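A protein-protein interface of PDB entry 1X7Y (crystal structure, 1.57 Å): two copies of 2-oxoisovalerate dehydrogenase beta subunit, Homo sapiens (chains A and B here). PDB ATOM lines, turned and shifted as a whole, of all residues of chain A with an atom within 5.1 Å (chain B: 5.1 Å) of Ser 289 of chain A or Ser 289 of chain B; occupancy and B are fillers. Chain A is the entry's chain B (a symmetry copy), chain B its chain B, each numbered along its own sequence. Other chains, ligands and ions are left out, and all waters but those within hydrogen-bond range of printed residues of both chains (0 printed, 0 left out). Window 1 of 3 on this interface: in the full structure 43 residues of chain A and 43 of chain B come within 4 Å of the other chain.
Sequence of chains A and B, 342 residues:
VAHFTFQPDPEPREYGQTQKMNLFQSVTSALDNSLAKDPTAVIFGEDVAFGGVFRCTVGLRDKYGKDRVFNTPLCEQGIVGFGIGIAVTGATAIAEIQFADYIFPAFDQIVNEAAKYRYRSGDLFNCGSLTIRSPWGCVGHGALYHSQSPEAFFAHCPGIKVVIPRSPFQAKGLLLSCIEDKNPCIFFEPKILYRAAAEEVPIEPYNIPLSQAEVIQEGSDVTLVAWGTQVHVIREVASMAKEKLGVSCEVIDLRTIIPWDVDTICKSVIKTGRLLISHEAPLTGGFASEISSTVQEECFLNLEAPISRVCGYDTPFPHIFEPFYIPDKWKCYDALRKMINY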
ATOM      1  N   HIS A 279     -16.603   9.445 -12.085  1.00  0.00           N
ATOM      2  CA  HIS A 279     -15.826  10.509 -11.496  1.00  0.00           C
ATOM      3  C   HIS A 279     -16.033  11.861 -12.172  1.00  0.00           C
ATOM      4  O   HIS A 279     -16.360  11.924 -13.365  1.00  0.00           O
ATOM      5  CB  HIS A 279     -14.323  10.152 -11.491  1.00  0.00           C
ATOM      6  CG  HIS A 279     -13.707   9.885 -12.851  1.00  0.00           C
ATOM      7  ND1 HIS A 279     -13.017   8.723 -13.168  1.00  0.00           N
ATOM      8  CD2 HIS A 279     -13.511  10.723 -13.900  1.00  0.00           C
ATOM      9  CE1 HIS A 279     -12.483   8.843 -14.392  1.00  0.00           C
ATOM     10  NE2 HIS A 279     -12.773  10.048 -14.850  1.00  0.00           N
ATOM     11  N   GLY A 285      -8.528   9.477 -20.418  1.00  0.00           N
ATOM     12  CA  GLY A 285      -7.341   9.380 -19.545  1.00  0.00           C
ATOM     13  C   GLY A 285      -7.684   9.493 -18.075  1.00  0.00           C
ATOM     14  O   GLY A 285      -6.782   9.469 -17.214  1.00  0.00           O
ATOM     15  N   GLY A 286      -8.989   9.552 -17.776  1.00  0.00           N
ATOM     16  CA  GLY A 286      -9.433   9.562 -16.359  1.00  0.00           C
ATOM     17  C   GLY A 286      -9.130   8.240 -15.668  1.00  0.00           C
ATOM     18  O   GLY A 286      -8.887   7.212 -16.330  1.00  0.00           O
ATOM     19  N   PHE A 287      -9.223   8.209 -14.345  1.00  0.00           N
ATOM     20  CA  PHE A 287      -8.816   6.978 -13.644  1.00  0.00           C
ATOM     21  C   PHE A 287      -9.815   5.835 -13.861  1.00  0.00           C
ATOM     22  O   PHE A 287      -9.472   4.674 -13.675  1.00  0.00           O
ATOM     23  CB  PHE A 287      -8.538   7.207 -12.140  1.00  0.00           C
ATOM     24  CG  PHE A 287      -7.783   6.069 -11.531  1.00  0.00           C
ATOM     25  CD1 PHE A 287      -6.467   5.823 -11.949  1.00  0.00           C
ATOM     26  CD2 PHE A 287      -8.383   5.228 -10.575  1.00  0.00           C
ATOM     27  CE1 PHE A 287      -5.737   4.710 -11.417  1.00  0.00           C
ATOM     28  CE2 PHE A 287      -7.686   4.127 -10.038  1.00  0.00           C
ATOM     29  CZ  PHE A 287      -6.380   3.876 -10.440  1.00  0.00           C
ATOM     30  N   ALA A 288     -11.067   6.147 -14.240  1.00  0.00           N
ATOM     31  CA  ALA A 288     -12.029   5.091 -14.590  1.00  0.00           C
ATOM     32  C   ALA A 288     -11.484   4.178 -15.691  1.00  0.00           C
ATOM     33  O   ALA A 288     -11.796   3.007 -15.720  1.00  0.00           O
ATOM     34  CB  ALA A 288     -13.412   5.659 -14.976  1.00  0.00           C
ATOM     35  N   SER A 289     -10.662   4.716 -16.587  1.00  0.00           N
ATOM     36  CA  SER A 289     -10.113   3.894 -17.679  1.00  0.00           C
ATOM     37  C   SER A 289      -9.192   2.803 -17.130  1.00  0.00           C
ATOM     38  O   SER A 289      -9.210   1.669 -17.621  1.00  0.00           O
ATOM     39  CB  SER A 289      -9.391   4.759 -18.718  1.00  0.00           C
ATOM     40  OG  SER A 289      -8.189   5.283 -18.200  1.00  0.00           O
ATOM     41  N   GLU A 290      -8.413   3.130 -16.100  1.00  0.00           N
ATOM     42  CA  GLU A 290      -7.533   2.122 -15.463  1.00  0.00           C
ATOM     43  C   GLU A 290      -8.294   1.044 -14.745  1.00  0.00           C
ATOM     44  O   GLU A 290      -7.996  -0.156 -14.921  1.00  0.00           O
ATOM     45  CB  GLU A 290      -6.530   2.759 -14.517  1.00  0.00           C
ATOM     46  CG  GLU A 290      -5.522   1.751 -13.930  1.00  0.00           C
ATOM     47  CD  GLU A 290      -4.667   1.030 -14.963  1.00  0.00           C
ATOM     48  OE1 GLU A 290      -4.247   1.684 -15.921  1.00  0.00           O
ATOM     49  OE2 GLU A 290      -4.511  -0.195 -14.836  1.00  0.00           O
ATOM     50  N   ILE A 291      -9.323   1.441 -14.015  1.00  0.00           N
ATOM     51  CA  ILE A 291     -10.176   0.450 -13.304  1.00  0.00           C
ATOM     52  C   ILE A 291     -10.897  -0.443 -14.304  1.00  0.00           C
ATOM     53  O   ILE A 291     -10.935  -1.677 -14.150  1.00  0.00           O
ATOM     54  CB  ILE A 291     -11.184   1.174 -12.364  1.00  0.00           C
ATOM     55  CG1 ILE A 291     -10.393   1.973 -11.305  1.00  0.00           C
ATOM     56  CG2 ILE A 291     -12.164   0.127 -11.703  1.00  0.00           C
ATOM     57  CD1 ILE A 291     -11.305   2.977 -10.473  1.00  0.00           C
ATOM     58  N   SER A 292     -11.458   0.169 -15.336  1.00  0.00           N
ATOM     59  CA  SER A 292     -12.226  -0.568 -16.351  1.00  0.00           C
ATOM     60  C   SER A 292     -11.323  -1.607 -17.050  1.00  0.00           C
ATOM     61  O   SER A 292     -11.656  -2.780 -17.101  1.00  0.00           O
ATOM     62  CB  SER A 292     -12.815   0.419 -17.396  1.00  0.00           C
ATOM     63  OG  SER A 292     -13.489  -0.354 -18.417  1.00  0.00           O
ATOM     64  N   SER A 293     -10.178  -1.155 -17.556  1.00  0.00           N
ATOM     65  CA  SER A 293      -9.249  -2.066 -18.235  1.00  0.00           C
ATOM     66  C   SER A 293      -8.745  -3.228 -17.350  1.00  0.00           C
ATOM     67  O   SER A 293      -8.617  -4.357 -17.839  1.00  0.00           O
ATOM     68  CB  SER A 293      -8.090  -1.285 -18.884  1.00  0.00           C
ATOM     69  OG  SER A 293      -7.368  -0.527 -17.938  1.00  0.00           O
ATOM     70  N   THR A 294      -8.487  -2.966 -16.067  1.00  0.00           N
ATOM     71  CA  THR A 294      -8.054  -3.997 -15.138  1.00  0.00           C
ATOM     72  C   THR A 294      -9.156  -4.992 -14.828  1.00  0.00           C
ATOM     73  O   THR A 294      -8.905  -6.207 -14.792  1.00  0.00           O
ATOM     74  CB  THR A 294      -7.555  -3.327 -13.859  1.00  0.00           C
ATOM     75  OG1 THR A 294      -6.383  -2.558 -14.164  1.00  0.00           O
ATOM     76  CG2 THR A 294      -7.072  -4.340 -12.843  1.00  0.00           C
ATOM     77  N   ARG A 309     -18.438   4.027 -17.925  1.00  0.00           N
ATOM     78  CA  ARG A 309     -17.740   5.130 -17.275  1.00  0.00           C
ATOM     79  C   ARG A 309     -18.599   6.374 -17.426  1.00  0.00           C
ATOM     80  O   ARG A 309     -18.927   6.760 -18.543  1.00  0.00           O
ATOM     81  CB  ARG A 309     -16.391   5.380 -17.914  1.00  0.00           C
ATOM     82  CG  ARG A 309     -15.429   4.230 -17.776  1.00  0.00           C
ATOM     83  CD  ARG A 309     -14.066   4.536 -18.441  1.00  0.00           C
ATOM     84  NE  ARG A 309     -14.139   4.618 -19.904  1.00  0.00           N
ATOM     85  CZ  ARG A 309     -13.225   5.288 -20.619  1.00  0.00           C
ATOM     86  NH1 ARG A 309     -12.277   5.992 -19.996  1.00  0.00           N
ATOM     87  NH2 ARG A 309     -13.312   5.295 -21.922  1.00  0.00           N
ATOM     88  N   HIS B 279       2.923  -0.298 -25.002  1.00  0.00           N
ATOM     89  CA  HIS B 279       3.717   0.904 -24.924  1.00  0.00           C
ATOM     90  C   HIS B 279       4.818   0.839 -23.868  1.00  0.00           C
ATOM     91  O   HIS B 279       4.689   0.119 -22.869  1.00  0.00           O
ATOM     92  CB  HIS B 279       2.823   2.137 -24.671  1.00  0.00           C
ATOM     93  CG  HIS B 279       1.994   2.098 -23.400  1.00  0.00           C
ATOM     94  ND1 HIS B 279       0.617   2.269 -23.375  1.00  0.00           N
ATOM     95  CD2 HIS B 279       2.387   2.108 -22.102  1.00  0.00           C
ATOM     96  CE1 HIS B 279       0.198   2.315 -22.102  1.00  0.00           C
ATOM     97  NE2 HIS B 279       1.257   2.219 -21.318  1.00  0.00           N
ATOM     98  N   GLY B 285      -2.337   3.727 -15.474  1.00  0.00           N
ATOM     99  CA  GLY B 285      -2.654   5.078 -15.978  1.00  0.00           C
ATOM    100  C   GLY B 285      -2.039   5.359 -17.332  1.00  0.00           C
ATOM    101  O   GLY B 285      -2.184   6.473 -17.872  1.00  0.00           O
ATOM    102  N   GLY B 286      -1.405   4.332 -17.916  1.00  0.00           N
ATOM    103  CA  GLY B 286      -0.855   4.474 -19.288  1.00  0.00           C
ATOM    104  C   GLY B 286      -1.963   4.637 -20.320  1.00  0.00           C
ATOM    105  O   GLY B 286      -3.138   4.320 -20.054  1.00  0.00           O
ATOM    106  N   PHE B 287      -1.609   5.043 -21.533  1.00  0.00           N
ATOM    107  CA  PHE B 287      -2.673   5.327 -22.512  1.00  0.00           C
ATOM    108  C   PHE B 287      -3.355   4.047 -23.009  1.00  0.00           C
ATOM    109  O   PHE B 287      -4.467   4.100 -23.522  1.00  0.00           O
ATOM    110  CB  PHE B 287      -2.186   6.202 -23.692  1.00  0.00           C
ATOM    111  CG  PHE B 287      -3.326   6.784 -24.464  1.00  0.00           C
ATOM    112  CD1 PHE B 287      -4.161   7.724 -23.842  1.00  0.00           C
ATOM    113  CD2 PHE B 287      -3.589   6.381 -25.787  1.00  0.00           C
ATOM    114  CE1 PHE B 287      -5.289   8.263 -24.543  1.00  0.00           C
ATOM    115  CE2 PHE B 287      -4.692   6.896 -26.497  1.00  0.00           C
ATOM    116  CZ  PHE B 287      -5.524   7.832 -25.893  1.00  0.00           C
ATOM    117  N   ALA B 288      -2.695   2.883 -22.881  1.00  0.00           N
ATOM    118  CA  ALA B 288      -3.349   1.609 -23.216  1.00  0.00           C
ATOM    119  C   ALA B 288      -4.654   1.426 -22.438  1.00  0.00           C
ATOM    120  O   ALA B 288      -5.577   0.817 -22.934  1.00  0.00           O
ATOM    121  CB  ALA B 288      -2.413   0.397 -23.021  1.00  0.00           C
ATOM    122  N   SER B 289      -4.728   1.965 -21.226  1.00  0.00           N
ATOM    123  CA  SER B 289      -5.952   1.815 -20.420  1.00  0.00           C
ATOM    124  C   SER B 289      -7.130   2.535 -21.078  1.00  0.00           C
ATOM    125  O   SER B 289      -8.255   2.022 -21.071  1.00  0.00           O
ATOM    126  CB  SER B 289      -5.736   2.301 -18.983  1.00  0.00           C
ATOM    127  OG  SER B 289      -5.602   3.705 -18.933  1.00  0.00           O
ATOM    128  N   GLU B 290      -6.873   3.702 -21.668  1.00  0.00           N
ATOM    129  CA  GLU B 290      -7.940   4.442 -22.384  1.00  0.00           C
ATOM    130  C   GLU B 290      -8.412   3.741 -23.626  1.00  0.00           C
ATOM    131  O   GLU B 290      -9.635   3.608 -23.842  1.00  0.00           O
ATOM    132  CB  GLU B 290      -7.516   5.860 -22.725  1.00  0.00           C
ATOM    133  CG  GLU B 290      -8.645   6.694 -23.364  1.00  0.00           C
ATOM    134  CD  GLU B 290      -9.882   6.864 -22.492  1.00  0.00           C
ATOM    135  OE1 GLU B 290      -9.715   7.057 -21.285  1.00  0.00           O
ATOM    136  OE2 GLU B 290     -10.993   6.713 -23.024  1.00  0.00           O
ATOM    137  N   ILE B 291      -7.473   3.214 -24.394  1.00  0.00           N
ATOM    138  CA  ILE B 291      -7.836   2.453 -25.621  1.00  0.00           C
ATOM    139  C   ILE B 291      -8.608   1.193 -25.255  1.00  0.00           C
ATOM    140  O   ILE B 291      -9.646   0.877 -25.865  1.00  0.00           O
ATOM    141  CB  ILE B 291      -6.561   2.113 -26.447  1.00  0.00           C
ATOM    142  CG1 ILE B 291      -5.884   3.431 -26.883  1.00  0.00           C
ATOM    143  CG2 ILE B 291      -6.937   1.206 -27.684  1.00  0.00           C
ATOM    144  CD1 ILE B 291      -4.427   3.213 -27.484  1.00  0.00           C
ATOM    145  N   SER B 292      -8.119   0.478 -24.253  1.00  0.00           N
ATOM    146  CA  SER B 292      -8.739  -0.786 -23.827  1.00  0.00           C
ATOM    147  C   SER B 292     -10.189  -0.536 -23.360  1.00  0.00           C
ATOM    148  O   SER B 292     -11.112  -1.173 -23.842  1.00  0.00           O
ATOM    149  CB  SER B 292      -7.911  -1.428 -22.681  1.00  0.00           C
ATOM    150  OG  SER B 292      -8.600  -2.620 -22.238  1.00  0.00           O
ATOM    151  N   SER B 293     -10.363   0.412 -22.442  1.00  0.00           N
ATOM    152  CA  SER B 293     -11.705   0.728 -21.938  1.00  0.00           C
ATOM    153  C   SER B 293     -12.697   1.186 -23.030  1.00  0.00           C
ATOM    154  O   SER B 293     -13.873   0.804 -22.986  1.00  0.00           O
ATOM    155  CB  SER B 293     -11.630   1.725 -20.765  1.00  0.00           C
ATOM    156  OG  SER B 293     -10.992   2.928 -21.134  1.00  0.00           O
ATOM    157  N   THR B 294     -12.231   1.968 -24.006  1.00  0.00           N
ATOM    158  CA  THR B 294     -13.069   2.416 -25.106  1.00  0.00           C
ATOM    159  C   THR B 294     -13.443   1.284 -26.043  1.00  0.00           C
ATOM    160  O   THR B 294     -14.605   1.184 -26.466  1.00  0.00           O
ATOM    161  CB  THR B 294     -12.335   3.523 -25.863  1.00  0.00           C
ATOM    162  OG1 THR B 294     -12.187   4.658 -24.997  1.00  0.00           O
ATOM    163  CG2 THR B 294     -13.153   4.053 -27.021  1.00  0.00           C
ATOM    164  N   ARG B 309      -2.685  -5.608 -22.319  1.00  0.00           N
ATOM    165  CA  ARG B 309      -1.809  -4.442 -22.302  1.00  0.00           C
ATOM    166  C   ARG B 309      -0.416  -4.917 -21.924  1.00  0.00           C
ATOM    167  O   ARG B 309      -0.239  -5.520 -20.871  1.00  0.00           O
ATOM    168  CB  ARG B 309      -2.275  -3.420 -21.288  1.00  0.00           C
ATOM    169  CG  ARG B 309      -3.628  -2.834 -21.592  1.00  0.00           C
ATOM    170  CD  ARG B 309      -4.057  -1.793 -20.531  1.00  0.00           C
ATOM    171  NE  ARG B 309      -4.337  -2.385 -19.217  1.00  0.00           N
ATOM    172  CZ  ARG B 309      -4.283  -1.659 -18.092  1.00  0.00           C
ATOM    173  NH1 ARG B 309      -3.864  -0.392 -18.134  1.00  0.00           N
ATOM    174  NH2 ARG B 309      -4.583  -2.223 -16.953  1.00  0.00           N
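OE1 of Glu 290 of chain A lies within hydrogen-bond range of N of Gly 285 of chain B.
The side-chain hydroxyl (OG) of Ser 289 of chain B lies within hydrogen-bond range of the side-chain hydroxyl (OG) of Ser 289 of chain A, at 3.1 Å.
The backbone NH of Gly 285 of chain A is in hydrogen-bond range of the side-chain carboxylate of Glu 290 of chain B.
NH2 of Arg 309 of chain A lies within salt-bridge range of OE2 of Glu 290 of chain B (2.9 Å).
OG of Ser 293 of chain B sits close to NH2 of Arg 309 of chain A (3.4 Å).
The side-chain hydroxyl (OG1) of Thr 294 of chain B lies within hydrogen-bond range of the guanidinium group (NH2) of Arg 309 of chain A (3.3 Å).
The side-chain carboxylate (OE2) of Glu 290 of chain A is in salt-bridge range of the guanidinium group (NH2) of Arg 309 of chain B (2.9 Å).
The guanidinium group (NH2) of Arg 309 of chain B sits close to the side-chain hydroxyl (OG) of Ser 293 of chain A, 3.4 Å away.
OG1 of Thr 294 of chain A is in hydrogen-bond range of NH2 of Arg 309 of chain B, at 3.3 Å.
OG of Ser 289 of chain B sits at hydrogen-bond distance from O of Gly 286 of chain B, 2.8 Å away.
The backbone carbonyl oxygen (O) of Ser 289 of chain B lies within hydrogen-bond range of the side-chain hydroxyl (OG) of Ser 293 of chain B (2.9 Å).
O of Glu 290 of chain B sits at hydrogen-bond distance from OG of Ser 293 of chain B, at 3.1 Å.
The backbone carbonyl oxygen (O) of Glu 290 of chain B lies within hydrogen-bond range of the side-chain hydroxyl (OG1) of Thr 294 of chain B, 3.0 Å away.
The side-chain hydroxyl (OG) of Ser 289 of chain A lies within hydrogen-bond range of the backbone carbonyl oxygen (O) of Gly 286 of chain A (2.8 Å).
O of Glu 290 of chain A sits at hydrogen-bond distance from OG of Ser 293 of chain A (3.1 Å).
Among the printed residues, pairs that only touch across the chains: Ser 289 of chain A with Ser 293 of chain B, Ser 293 of chain A with Ser 289 of chain B, Glu 290 of chain A with Ser 289 of chain B, Ser 289 of chain A with Glu 290 of chain B, Ser 292 of chain A with Ser 293 of chain B and Ser 293 of chain A with Ser 292 of chain B.
Of the printed residues of chain B, Ser 293 of chain A touches Ser 289, Ser 292 and Arg 309.
Printed residues of chain B within 4 Å of Thr 294 of chain A: Arg 309.
Of the printed residues of chain A, Glu 290 of chain B touches Gly 285 (2.8 Å), Ser 289 (3.5 Å) and Arg 309 (2.9 Å).
Ile 291 of chain B touches none of the printed residues of chain A.
Of the printed residues of chain A, Ser 292 of chain B touches Ser 293 (3.6 Å).
Of the printed residues of chain A, Arg 309 of chain B touches Glu 290 (2.9 Å), Ser 293 (3.3 Å) and Thr 294 (3.3 Å).
The nearest printed residue of chain A that does not touch Ser 289 of chain B is Gly 286 of chain A (5.5 Å).
Of the 12 printed residues of chain B, 7 touch a printed residue of chain A.
Glu 290 of chain A touches Arg 309 of chain B, and with the chains exchanged Arg 309 of chain A touches Glu 290 of chain B.
Ser 292 of chain A touches Ser 293 of chain B, and with the chains exchanged Ser 293 of chain A touches Ser 292 of chain B.
Ser 293 of chain A touches Arg 309 of chain B, and with the chains exchanged Arg 309 of chain A touches Ser 293 of chain B.
Thr 294 of chain A touches Arg 309 of chain B, and with the chains exchanged Arg 309 of chain A touches Thr 294 of chain B.
Positions printed for both chains: 279, 285, 286, 287, 288, 289, 290, 291, 292, 293, 294 and 309.
Of the 15 pairs that touch across the chains among the printed residues, 15 have their exchanged pair printed and touching as well.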
